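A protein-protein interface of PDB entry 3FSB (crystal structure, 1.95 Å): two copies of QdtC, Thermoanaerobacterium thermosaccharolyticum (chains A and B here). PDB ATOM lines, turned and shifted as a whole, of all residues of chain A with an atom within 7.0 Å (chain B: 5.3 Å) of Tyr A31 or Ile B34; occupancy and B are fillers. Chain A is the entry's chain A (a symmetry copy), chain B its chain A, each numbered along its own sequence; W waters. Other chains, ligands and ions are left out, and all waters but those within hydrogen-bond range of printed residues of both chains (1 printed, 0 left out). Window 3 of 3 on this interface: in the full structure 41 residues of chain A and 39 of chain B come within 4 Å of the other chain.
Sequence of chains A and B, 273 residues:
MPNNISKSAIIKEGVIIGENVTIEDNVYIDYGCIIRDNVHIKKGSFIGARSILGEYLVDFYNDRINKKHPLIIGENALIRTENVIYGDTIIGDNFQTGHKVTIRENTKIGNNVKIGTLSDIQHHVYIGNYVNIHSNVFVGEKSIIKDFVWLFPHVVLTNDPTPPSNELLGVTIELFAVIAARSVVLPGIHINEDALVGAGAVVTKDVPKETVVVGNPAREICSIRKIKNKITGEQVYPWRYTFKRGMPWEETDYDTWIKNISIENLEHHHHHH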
ATOM      1  N   ILE A  11      -9.357 -28.647  27.224  1.00  0.00           N
ATOM      2  CA  ILE A  11      -8.428 -27.533  27.094  1.00  0.00           C
ATOM      3  C   ILE A  11      -7.169 -27.873  27.882  1.00  0.00           C
ATOM      4  O   ILE A  11      -7.221 -27.938  29.103  1.00  0.00           O
ATOM      5  CB  ILE A  11      -9.048 -26.229  27.648  1.00  0.00           C
ATOM      6  CG1 ILE A  11     -10.407 -25.885  27.048  1.00  0.00           C
ATOM      7  CG2 ILE A  11      -8.060 -25.044  27.539  1.00  0.00           C
ATOM      8  CD1 ILE A  11     -10.624 -26.426  25.652  1.00  0.00           C
ATOM      9  N   LYS A  12      -6.060 -28.119  27.185  1.00  0.00           N
ATOM     10  CA  LYS A  12      -4.797 -28.478  27.836  1.00  0.00           C
ATOM     11  C   LYS A  12      -4.157 -27.281  28.519  1.00  0.00           C
ATOM     12  O   LYS A  12      -4.579 -26.136  28.386  1.00  0.00           O
ATOM     13  CB  LYS A  12      -3.742 -29.003  26.838  1.00  0.00           C
ATOM     14  CG  LYS A  12      -4.034 -30.346  26.163  1.00  0.00           C
ATOM     15  CD  LYS A  12      -4.994 -31.274  26.890  1.00  0.00           C
ATOM     16  CE  LYS A  12      -4.300 -32.183  27.877  1.00  0.00           C
ATOM     17  NZ  LYS A  12      -4.652 -33.626  27.732  1.00  0.00           N
ATOM     18  N   GLU A  13      -3.059 -27.557  29.219  1.00  0.00           N
ATOM     19  CA  GLU A  13      -2.299 -26.549  29.922  1.00  0.00           C
ATOM     20  C   GLU A  13      -1.653 -25.565  28.945  1.00  0.00           C
ATOM     21  O   GLU A  13      -1.306 -25.873  27.794  1.00  0.00           O
ATOM     22  CB  GLU A  13      -1.280 -27.232  30.855  1.00  0.00           C
ATOM     23  CG  GLU A  13       0.177 -26.898  30.655  1.00  0.00           C
ATOM     24  CD  GLU A  13       0.952 -26.816  31.960  1.00  0.00           C
ATOM     25  OE1 GLU A  13       1.089 -27.849  32.642  1.00  0.00           O
ATOM     26  OE2 GLU A  13       1.385 -25.687  32.315  1.00  0.00           O
ATOM     27  N   GLY A  14      -1.531 -24.339  29.439  1.00  0.00           N
ATOM     28  CA  GLY A  14      -0.900 -23.272  28.676  1.00  0.00           C
ATOM     29  C   GLY A  14      -1.816 -22.511  27.745  1.00  0.00           C
ATOM     30  O   GLY A  14      -1.447 -21.442  27.243  1.00  0.00           O
ATOM     31  N   VAL A  15      -2.996 -23.078  27.530  1.00  0.00           N
ATOM     32  CA  VAL A  15      -3.911 -22.373  26.644  1.00  0.00           C
ATOM     33  C   VAL A  15      -4.295 -20.986  27.196  1.00  0.00           C
ATOM     34  O   VAL A  15      -4.557 -20.808  28.390  1.00  0.00           O
ATOM     35  CB  VAL A  15      -5.132 -23.236  26.296  1.00  0.00           C
ATOM     36  CG1 VAL A  15      -6.112 -22.431  25.493  1.00  0.00           C
ATOM     37  CG2 VAL A  15      -4.696 -24.519  25.571  1.00  0.00           C
ATOM     38  N   TYR A  28     -10.970 -30.091  21.357  1.00  0.00           N
ATOM     39  CA  TYR A  28      -9.792 -30.426  22.117  1.00  0.00           C
ATOM     40  C   TYR A  28      -8.839 -29.337  21.679  1.00  0.00           C
ATOM     41  O   TYR A  28      -8.566 -29.193  20.498  1.00  0.00           O
ATOM     42  CB  TYR A  28      -9.271 -31.790  21.646  1.00  0.00           C
ATOM     43  CG  TYR A  28      -8.061 -32.294  22.401  1.00  0.00           C
ATOM     44  CD1 TYR A  28      -8.089 -33.519  23.054  1.00  0.00           C
ATOM     45  CD2 TYR A  28      -6.890 -31.544  22.455  1.00  0.00           C
ATOM     46  CE1 TYR A  28      -6.983 -33.987  23.766  1.00  0.00           C
ATOM     47  CE2 TYR A  28      -5.797 -31.977  23.163  1.00  0.00           C
ATOM     48  CZ  TYR A  28      -5.849 -33.209  23.804  1.00  0.00           C
ATOM     49  OH  TYR A  28      -4.793 -33.719  24.508  1.00  0.00           O
ATOM     50  N   ILE A  29      -8.362 -28.557  22.632  1.00  0.00           N
ATOM     51  CA  ILE A  29      -7.423 -27.482  22.348  1.00  0.00           C
ATOM     52  C   ILE A  29      -6.106 -27.829  22.992  1.00  0.00           C
ATOM     53  O   ILE A  29      -5.964 -27.816  24.206  1.00  0.00           O
ATOM     54  CB  ILE A  29      -7.992 -26.186  22.810  1.00  0.00           C
ATOM     55  CG1 ILE A  29      -9.266 -25.994  21.993  1.00  0.00           C
ATOM     56  CG2 ILE A  29      -6.987 -25.076  22.618  1.00  0.00           C
ATOM     57  CD1 ILE A  29      -9.832 -24.668  22.172  1.00  0.00           C
ATOM     58  N   ASP A  30      -5.162 -28.203  22.145  1.00  0.00           N
ATOM     59  CA  ASP A  30      -3.865 -28.628  22.622  1.00  0.00           C
ATOM     60  C   ASP A  30      -2.979 -27.604  23.357  1.00  0.00           C
ATOM     61  O   ASP A  30      -3.254 -26.393  23.344  1.00  0.00           O
ATOM     62  CB  ASP A  30      -3.200 -29.562  21.588  1.00  0.00           C
ATOM     63  CG  ASP A  30      -2.214 -30.557  22.198  1.00  0.00           C
ATOM     64  OD1 ASP A  30      -2.055 -30.599  23.451  1.00  0.00           O
ATOM     65  OD2 ASP A  30      -1.536 -31.283  21.423  1.00  0.00           O
ATOM     66  N   TYR A  31      -1.924 -28.103  24.005  1.00  0.00           N
ATOM     67  CA  TYR A  31      -0.990 -27.266  24.766  1.00  0.00           C
ATOM     68  C   TYR A  31      -0.589 -25.962  24.143  1.00  0.00           C
ATOM     69  O   TYR A  31      -0.172 -25.880  22.981  1.00  0.00           O
ATOM     70  CB  TYR A  31       0.326 -27.979  25.102  1.00  0.00           C
ATOM     71  CG  TYR A  31       0.185 -29.236  25.903  1.00  0.00           C
ATOM     72  CD1 TYR A  31      -0.238 -29.195  27.243  1.00  0.00           C
ATOM     73  CD2 TYR A  31       0.491 -30.465  25.323  1.00  0.00           C
ATOM     74  CE1 TYR A  31      -0.353 -30.359  27.984  1.00  0.00           C
ATOM     75  CE2 TYR A  31       0.371 -31.633  26.063  1.00  0.00           C
ATOM     76  CZ  TYR A  31      -0.067 -31.565  27.376  1.00  0.00           C
ATOM     77  OH  TYR A  31      -0.185 -32.724  28.097  1.00  0.00           O
ATOM     78  N   GLY A  32      -0.675 -24.968  25.008  1.00  0.00           N
ATOM     79  CA  GLY A  32      -0.292 -23.621  24.689  1.00  0.00           C
ATOM     80  C   GLY A  32      -0.920 -22.824  23.564  1.00  0.00           C
ATOM     81  O   GLY A  32      -0.326 -21.835  23.135  1.00  0.00           O
ATOM     82  N   CYS A  33      -2.090 -23.221  23.083  1.00  0.00           N
ATOM     83  CA  CYS A  33      -2.697 -22.442  22.006  1.00  0.00           C
ATOM     84  C   CYS A  33      -3.075 -21.068  22.528  1.00  0.00           C
ATOM     85  O   CYS A  33      -3.344 -20.868  23.721  1.00  0.00           O
ATOM     86  CB  CYS A  33      -4.022 -23.058  21.630  1.00  0.00           C
ATOM     87  SG  CYS A  33      -3.767 -24.469  20.538  1.00  0.00           S
ATOM     88  N   ILE A  34      -3.126 -20.108  21.631  1.00  0.00           N
ATOM     89  CA  ILE A  34      -3.541 -18.805  22.093  1.00  0.00           C
ATOM     90  C   ILE A  34      -4.818 -18.554  21.293  1.00  0.00           C
ATOM     91  O   ILE A  34      -4.828 -18.597  20.054  1.00  0.00           O
ATOM     92  CB  ILE A  34      -2.580 -17.644  21.850  1.00  0.00           C
ATOM     93  CG1 ILE A  34      -1.256 -17.805  22.580  1.00  0.00           C
ATOM     94  CG2 ILE A  34      -3.323 -16.333  22.056  1.00  0.00           C
ATOM     95  CD1 ILE A  34      -0.150 -16.878  21.976  1.00  0.00           C
ATOM     96  N   ILE A  47      -7.610 -28.508  17.840  1.00  0.00           N
ATOM     97  CA  ILE A  47      -6.699 -27.386  17.571  1.00  0.00           C
ATOM     98  C   ILE A  47      -5.268 -27.692  18.048  1.00  0.00           C
ATOM     99  O   ILE A  47      -5.014 -27.842  19.224  1.00  0.00           O
ATOM    100  CB  ILE A  47      -7.197 -26.094  18.190  1.00  0.00           C
ATOM    101  CG1 ILE A  47      -8.660 -25.807  17.834  1.00  0.00           C
ATOM    102  CG2 ILE A  47      -6.292 -24.976  17.816  1.00  0.00           C
ATOM    103  CD1 ILE A  47      -9.031 -25.547  16.343  1.00  0.00           C
ATOM    104  N   GLY A  48      -4.325 -27.800  17.117  1.00  0.00           N
ATOM    105  CA  GLY A  48      -2.937 -28.129  17.418  1.00  0.00           C
ATOM    106  C   GLY A  48      -2.132 -27.229  18.353  1.00  0.00           C
ATOM    107  O   GLY A  48      -2.297 -26.004  18.462  1.00  0.00           O
ATOM    108  N   ALA A  49      -1.187 -27.883  19.004  1.00  0.00           N
ATOM    109  CA  ALA A  49      -0.366 -27.171  19.958  1.00  0.00           C
ATOM    110  C   ALA A  49       0.152 -25.815  19.522  1.00  0.00           C
ATOM    111  O   ALA A  49       0.681 -25.632  18.427  1.00  0.00           O
ATOM    112  CB  ALA A  49       0.736 -28.092  20.465  1.00  0.00           C
ATOM    113  N   ARG A  50       0.017 -24.856  20.416  1.00  0.00           N
ATOM    114  CA  ARG A  50       0.535 -23.533  20.129  1.00  0.00           C
ATOM    115  C   ARG A  50      -0.024 -22.806  18.922  1.00  0.00           C
ATOM    116  O   ARG A  50       0.530 -21.790  18.514  1.00  0.00           O
ATOM    117  CB  ARG A  50       2.074 -23.565  20.114  1.00  0.00           C
ATOM    118  CG  ARG A  50       2.681 -23.801  21.517  1.00  0.00           C
ATOM    119  CD  ARG A  50       4.201 -23.607  21.621  1.00  0.00           C
ATOM    120  NE  ARG A  50       4.984 -24.847  21.644  1.00  0.00           N
ATOM    121  CZ  ARG A  50       5.184 -25.631  22.701  1.00  0.00           C
ATOM    122  NH1 ARG A  50       4.653 -25.357  23.895  1.00  0.00           N
ATOM    123  NH2 ARG A  50       5.920 -26.721  22.540  1.00  0.00           N
ATOM    124  N   SER A  51      -1.128 -23.274  18.357  1.00  0.00           N
ATOM    125  CA  SER A  51      -1.654 -22.510  17.237  1.00  0.00           C
ATOM    126  C   SER A  51      -2.074 -21.196  17.883  1.00  0.00           C
ATOM    127  O   SER A  51      -2.127 -21.081  19.119  1.00  0.00           O
ATOM    128  CB  SER A  51      -2.910 -23.169  16.640  1.00  0.00           C
ATOM    129  OG  SER A  51      -2.557 -24.324  15.911  1.00  0.00           O
ATOM    130  N   THR A  81      -0.253 -28.453  14.605  1.00  0.00           N
ATOM    131  CA  THR A  81       0.480 -27.469  15.375  1.00  0.00           C
ATOM    132  C   THR A  81       0.858 -26.127  14.811  1.00  0.00           C
ATOM    133  O   THR A  81       1.118 -25.990  13.621  1.00  0.00           O
ATOM    134  CB  THR A  81       1.731 -28.028  16.119  1.00  0.00           C
ATOM    135  OG1 THR A  81       2.804 -28.131  15.183  1.00  0.00           O
ATOM    136  CG2 THR A  81       1.489 -29.398  16.798  1.00  0.00           C
ATOM    137  N   ILE B  16       6.979 -30.005  28.695  1.00  0.00           N
ATOM    138  CA  ILE B  16       5.890 -30.903  29.061  1.00  0.00           C
ATOM    139  C   ILE B  16       6.356 -32.282  28.629  1.00  0.00           C
ATOM    140  O   ILE B  16       6.811 -32.474  27.489  1.00  0.00           O
ATOM    141  CB  ILE B  16       4.569 -30.640  28.306  1.00  0.00           C
ATOM    142  CG1 ILE B  16       3.928 -29.335  28.759  1.00  0.00           C
ATOM    143  CG2 ILE B  16       3.580 -31.768  28.568  1.00  0.00           C
ATOM    144  CD1 ILE B  16       2.619 -29.574  29.483  1.00  0.00           C
ATOM    145  N   GLY B  32       9.945 -24.720  26.955  1.00  0.00           N
ATOM    146  CA  GLY B  32       8.692 -25.132  26.386  1.00  0.00           C
ATOM    147  C   GLY B  32       8.563 -26.284  25.410  1.00  0.00           C
ATOM    148  O   GLY B  32       7.549 -26.360  24.717  1.00  0.00           O
ATOM    149  N   CYS B  33       9.548 -27.167  25.339  1.00  0.00           N
ATOM    150  CA  CYS B  33       9.413 -28.283  24.405  1.00  0.00           C
ATOM    151  C   CYS B  33       8.276 -29.182  24.854  1.00  0.00           C
ATOM    152  O   CYS B  33       7.938 -29.272  26.043  1.00  0.00           O
ATOM    153  CB  CYS B  33      10.630 -29.168  24.504  1.00  0.00           C
ATOM    154  SG  CYS B  33      11.991 -28.466  23.554  1.00  0.00           S
ATOM    155  N   ILE B  34       7.691 -29.883  23.907  1.00  0.00           N
ATOM    156  CA  ILE B  34       6.647 -30.792  24.319  1.00  0.00           C
ATOM    157  C   ILE B  34       7.200 -32.153  23.903  1.00  0.00           C
ATOM    158  O   ILE B  34       7.541 -32.387  22.734  1.00  0.00           O
ATOM    159  CB  ILE B  34       5.274 -30.608  23.675  1.00  0.00           C
ATOM    160  CG1 ILE B  34       4.640 -29.265  24.001  1.00  0.00           C
ATOM    161  CG2 ILE B  34       4.434 -31.848  23.939  1.00  0.00           C
ATOM    162  CD1 ILE B  34       3.490 -28.915  22.998  1.00  0.00           C
ATOM    163  N   ILE B  35       7.340 -33.037  24.887  1.00  0.00           N
ATOM    164  CA  ILE B  35       7.834 -34.372  24.578  1.00  0.00           C
ATOM    165  C   ILE B  35       6.649 -35.300  24.837  1.00  0.00           C
ATOM    166  O   ILE B  35       6.268 -35.562  25.978  1.00  0.00           O
ATOM    167  CB  ILE B  35       8.965 -34.802  25.518  1.00  0.00           C
ATOM    168  CG1 ILE B  35      10.070 -33.762  25.550  1.00  0.00           C
ATOM    169  CG2 ILE B  35       9.693 -36.043  24.970  1.00  0.00           C
ATOM    170  CD1 ILE B  35      10.540 -33.401  24.159  1.00  0.00           C
ATOM    171  N   ARG B  36       6.045 -35.788  23.763  1.00  0.00           N
ATOM    172  CA  ARG B  36       4.900 -36.672  23.894  1.00  0.00           C
ATOM    173  C   ARG B  36       5.422 -38.054  24.240  1.00  0.00           C
ATOM    174  O   ARG B  36       6.635 -38.251  24.432  1.00  0.00           O
ATOM    175  CB  ARG B  36       4.030 -36.691  22.615  1.00  0.00           C
ATOM    176  CG  ARG B  36       3.772 -35.303  22.040  1.00  0.00           C
ATOM    177  CD  ARG B  36       2.426 -35.329  21.361  1.00  0.00           C
ATOM    178  NE  ARG B  36       2.214 -34.184  20.470  1.00  0.00           N
ATOM    179  CZ  ARG B  36       1.482 -33.128  20.792  1.00  0.00           C
ATOM    180  NH1 ARG B  36       1.323 -32.123  19.938  1.00  0.00           N
ATOM    181  NH2 ARG B  36       0.918 -33.060  21.983  1.00  0.00           N
ATOM    182  N   ARG B  50      10.647 -25.106  22.379  1.00  0.00           N
ATOM    183  CA  ARG B  50       9.346 -25.386  21.805  1.00  0.00           C
ATOM    184  C   ARG B  50       9.265 -26.460  20.738  1.00  0.00           C
ATOM    185  O   ARG B  50       8.241 -26.581  20.073  1.00  0.00           O
ATOM    186  CB  ARG B  50       8.684 -24.074  21.345  1.00  0.00           C
ATOM    187  CG  ARG B  50       8.274 -23.165  22.527  1.00  0.00           C
ATOM    188  CD  ARG B  50       7.396 -21.959  22.160  1.00  0.00           C
ATOM    189  NE  ARG B  50       8.103 -20.676  22.096  1.00  0.00           N
ATOM    190  CZ  ARG B  50       8.431 -19.906  23.130  1.00  0.00           C
ATOM    191  NH1 ARG B  50       8.145 -20.253  24.388  1.00  0.00           N
ATOM    192  NH2 ARG B  50       9.075 -18.773  22.887  1.00  0.00           N
ATOM    193  N   SER B  51      10.302 -27.271  20.577  1.00  0.00           N
ATOM    194  CA  SER B  51      10.153 -28.319  19.579  1.00  0.00           C
ATOM    195  C   SER B  51       9.058 -29.199  20.166  1.00  0.00           C
ATOM    196  O   SER B  51       8.683 -29.056  21.342  1.00  0.00           O
ATOM    197  CB  SER B  51      11.430 -29.168  19.454  1.00  0.00           C
ATOM    198  OG  SER B  51      12.439 -28.440  18.791  1.00  0.00           O
ATOM    199  N   ILE B  52       8.569 -30.134  19.363  1.00  0.00           N
ATOM    200  CA  ILE B  52       7.532 -31.055  19.845  1.00  0.00           C
ATOM    201  C   ILE B  52       7.988 -32.372  19.289  1.00  0.00           C
ATOM    202  O   ILE B  52       8.045 -32.545  18.068  1.00  0.00           O
ATOM    203  CB  ILE B  52       6.170 -30.742  19.179  1.00  0.00           C
ATOM    204  CG1 ILE B  52       5.782 -29.293  19.456  1.00  0.00           C
ATOM    205  CG2 ILE B  52       5.108 -31.745  19.602  1.00  0.00           C
ATOM    206  CD1 ILE B  52       4.370 -28.885  18.990  1.00  0.00           C
ATOM    207  N   LEU B  53       8.347 -33.283  20.183  1.00  0.00           N
ATOM    208  CA  LEU B  53       8.798 -34.599  19.768  1.00  0.00           C
ATOM    209  C   LEU B  53       7.770 -35.660  20.129  1.00  0.00           C
ATOM    210  O   LEU B  53       7.138 -35.608  21.184  1.00  0.00           O
ATOM    211  CB  LEU B  53      10.094 -34.927  20.469  1.00  0.00           C
ATOM    212  CG  LEU B  53      11.127 -33.813  20.423  1.00  0.00           C
ATOM    213  CD1 LEU B  53      12.413 -34.464  20.955  1.00  0.00           C
ATOM    214  CD2 LEU B  53      11.249 -33.421  18.960  1.00  0.00           C
HETATM  215  O   HOH W   1      -1.387 -30.939  18.994  1.00  0.00           O
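NH2 of Arg B36 lies within salt-bridge range of OD2 of Asp A30 (3.1 Å). O of Gly B32 sits at hydrogen-bond distance from NH2 of Arg A50 (2.7 Å). O of Arg B50 lies within hydrogen-bond range of NH2 of Arg A50, at 3.4 Å.
The backbone carbonyl oxygen of Ile B34 sits at hydrogen-bond distance from the backbone NH of Leu B53, 2.8 Å away. The backbone NH (N) of Ile B16 lies within hydrogen-bond range of the backbone carbonyl oxygen (O) of Cys B33, at 2.9 Å. The side-chain sulfur of Cys A33 lies within hydrogen-bond range of the backbone carbonyl oxygen of Asp A30. O of Ile B16 sits at hydrogen-bond distance from N of Ile B35 (2.7 Å). The backbone carbonyl oxygen of Ser B51 lies within hydrogen-bond range of the backbone NH of Ile B34 (2.9 Å). N of Arg A50 sits at hydrogen-bond distance from O of Tyr A31.
Among the printed residues, merely in contact across the chains: Arg A50 with Ile B34 (3.2 Å), Tyr A31 with Ile B16 (3.4 Å), Thr A81 with Ile B52 (3.7 Å), Glu A13 with Ile B16 (3.8 Å), Arg A50 with Ser B51 (3.8 Å), Ala A49 with Ile B34 (3.8 Å) and Tyr A31 with Ile B34 (3.9 Å).
Of chain B, only Ile B16 (3.4 Å) and Ile B34 (3.9 Å) come within 4 Å of Tyr A31. Ile B34 touches just these residues of chain A: Tyr A31 (3.9 Å), Ala A49 (3.8 Å) and Arg A50 (3.2 Å). Printed residues of chain A within 4 Å of Ile B52: Thr A81. Of the printed residues of chain B, Glu A13 touches Ile B16 (3.8 Å). The nearest residue of chain B that does not touch Tyr A31 is Arg B36 (4.3 Å). The nearest residue of chain A that does not touch Ile B34 is Asp A30 (5.8 Å). The nearest printed residue of chain B that does not touch Asp A30 is Ile B34 (5.8 Å).
Of the 10 printed residues of chain B, 7 touch a printed residue of chain A.
Arg A50 touches Gly B32, but with the chains exchanged Gly A32 does not touch Arg B50 (7.8 Å). Arg A50 touches Ile B34, but with the chains exchanged Ile A34 does not touch Arg B50 (9.1 Å). Arg B50 touches its own counterpart, Arg A50. Arg A50 touches Ser B51, but with the chains exchanged Ser A51 does not touch Arg B50 (9.4 Å). 5 positions are printed for both chains.
Water W1 lies within hydrogen-bond range of the side-chain carboxylate (OD2) of Asp A30 (2.5 Å), the backbone NH (N) of Ala A49 (3.1 Å) and the guanidinium group (NH1) of Arg B36 (3.1 Å).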
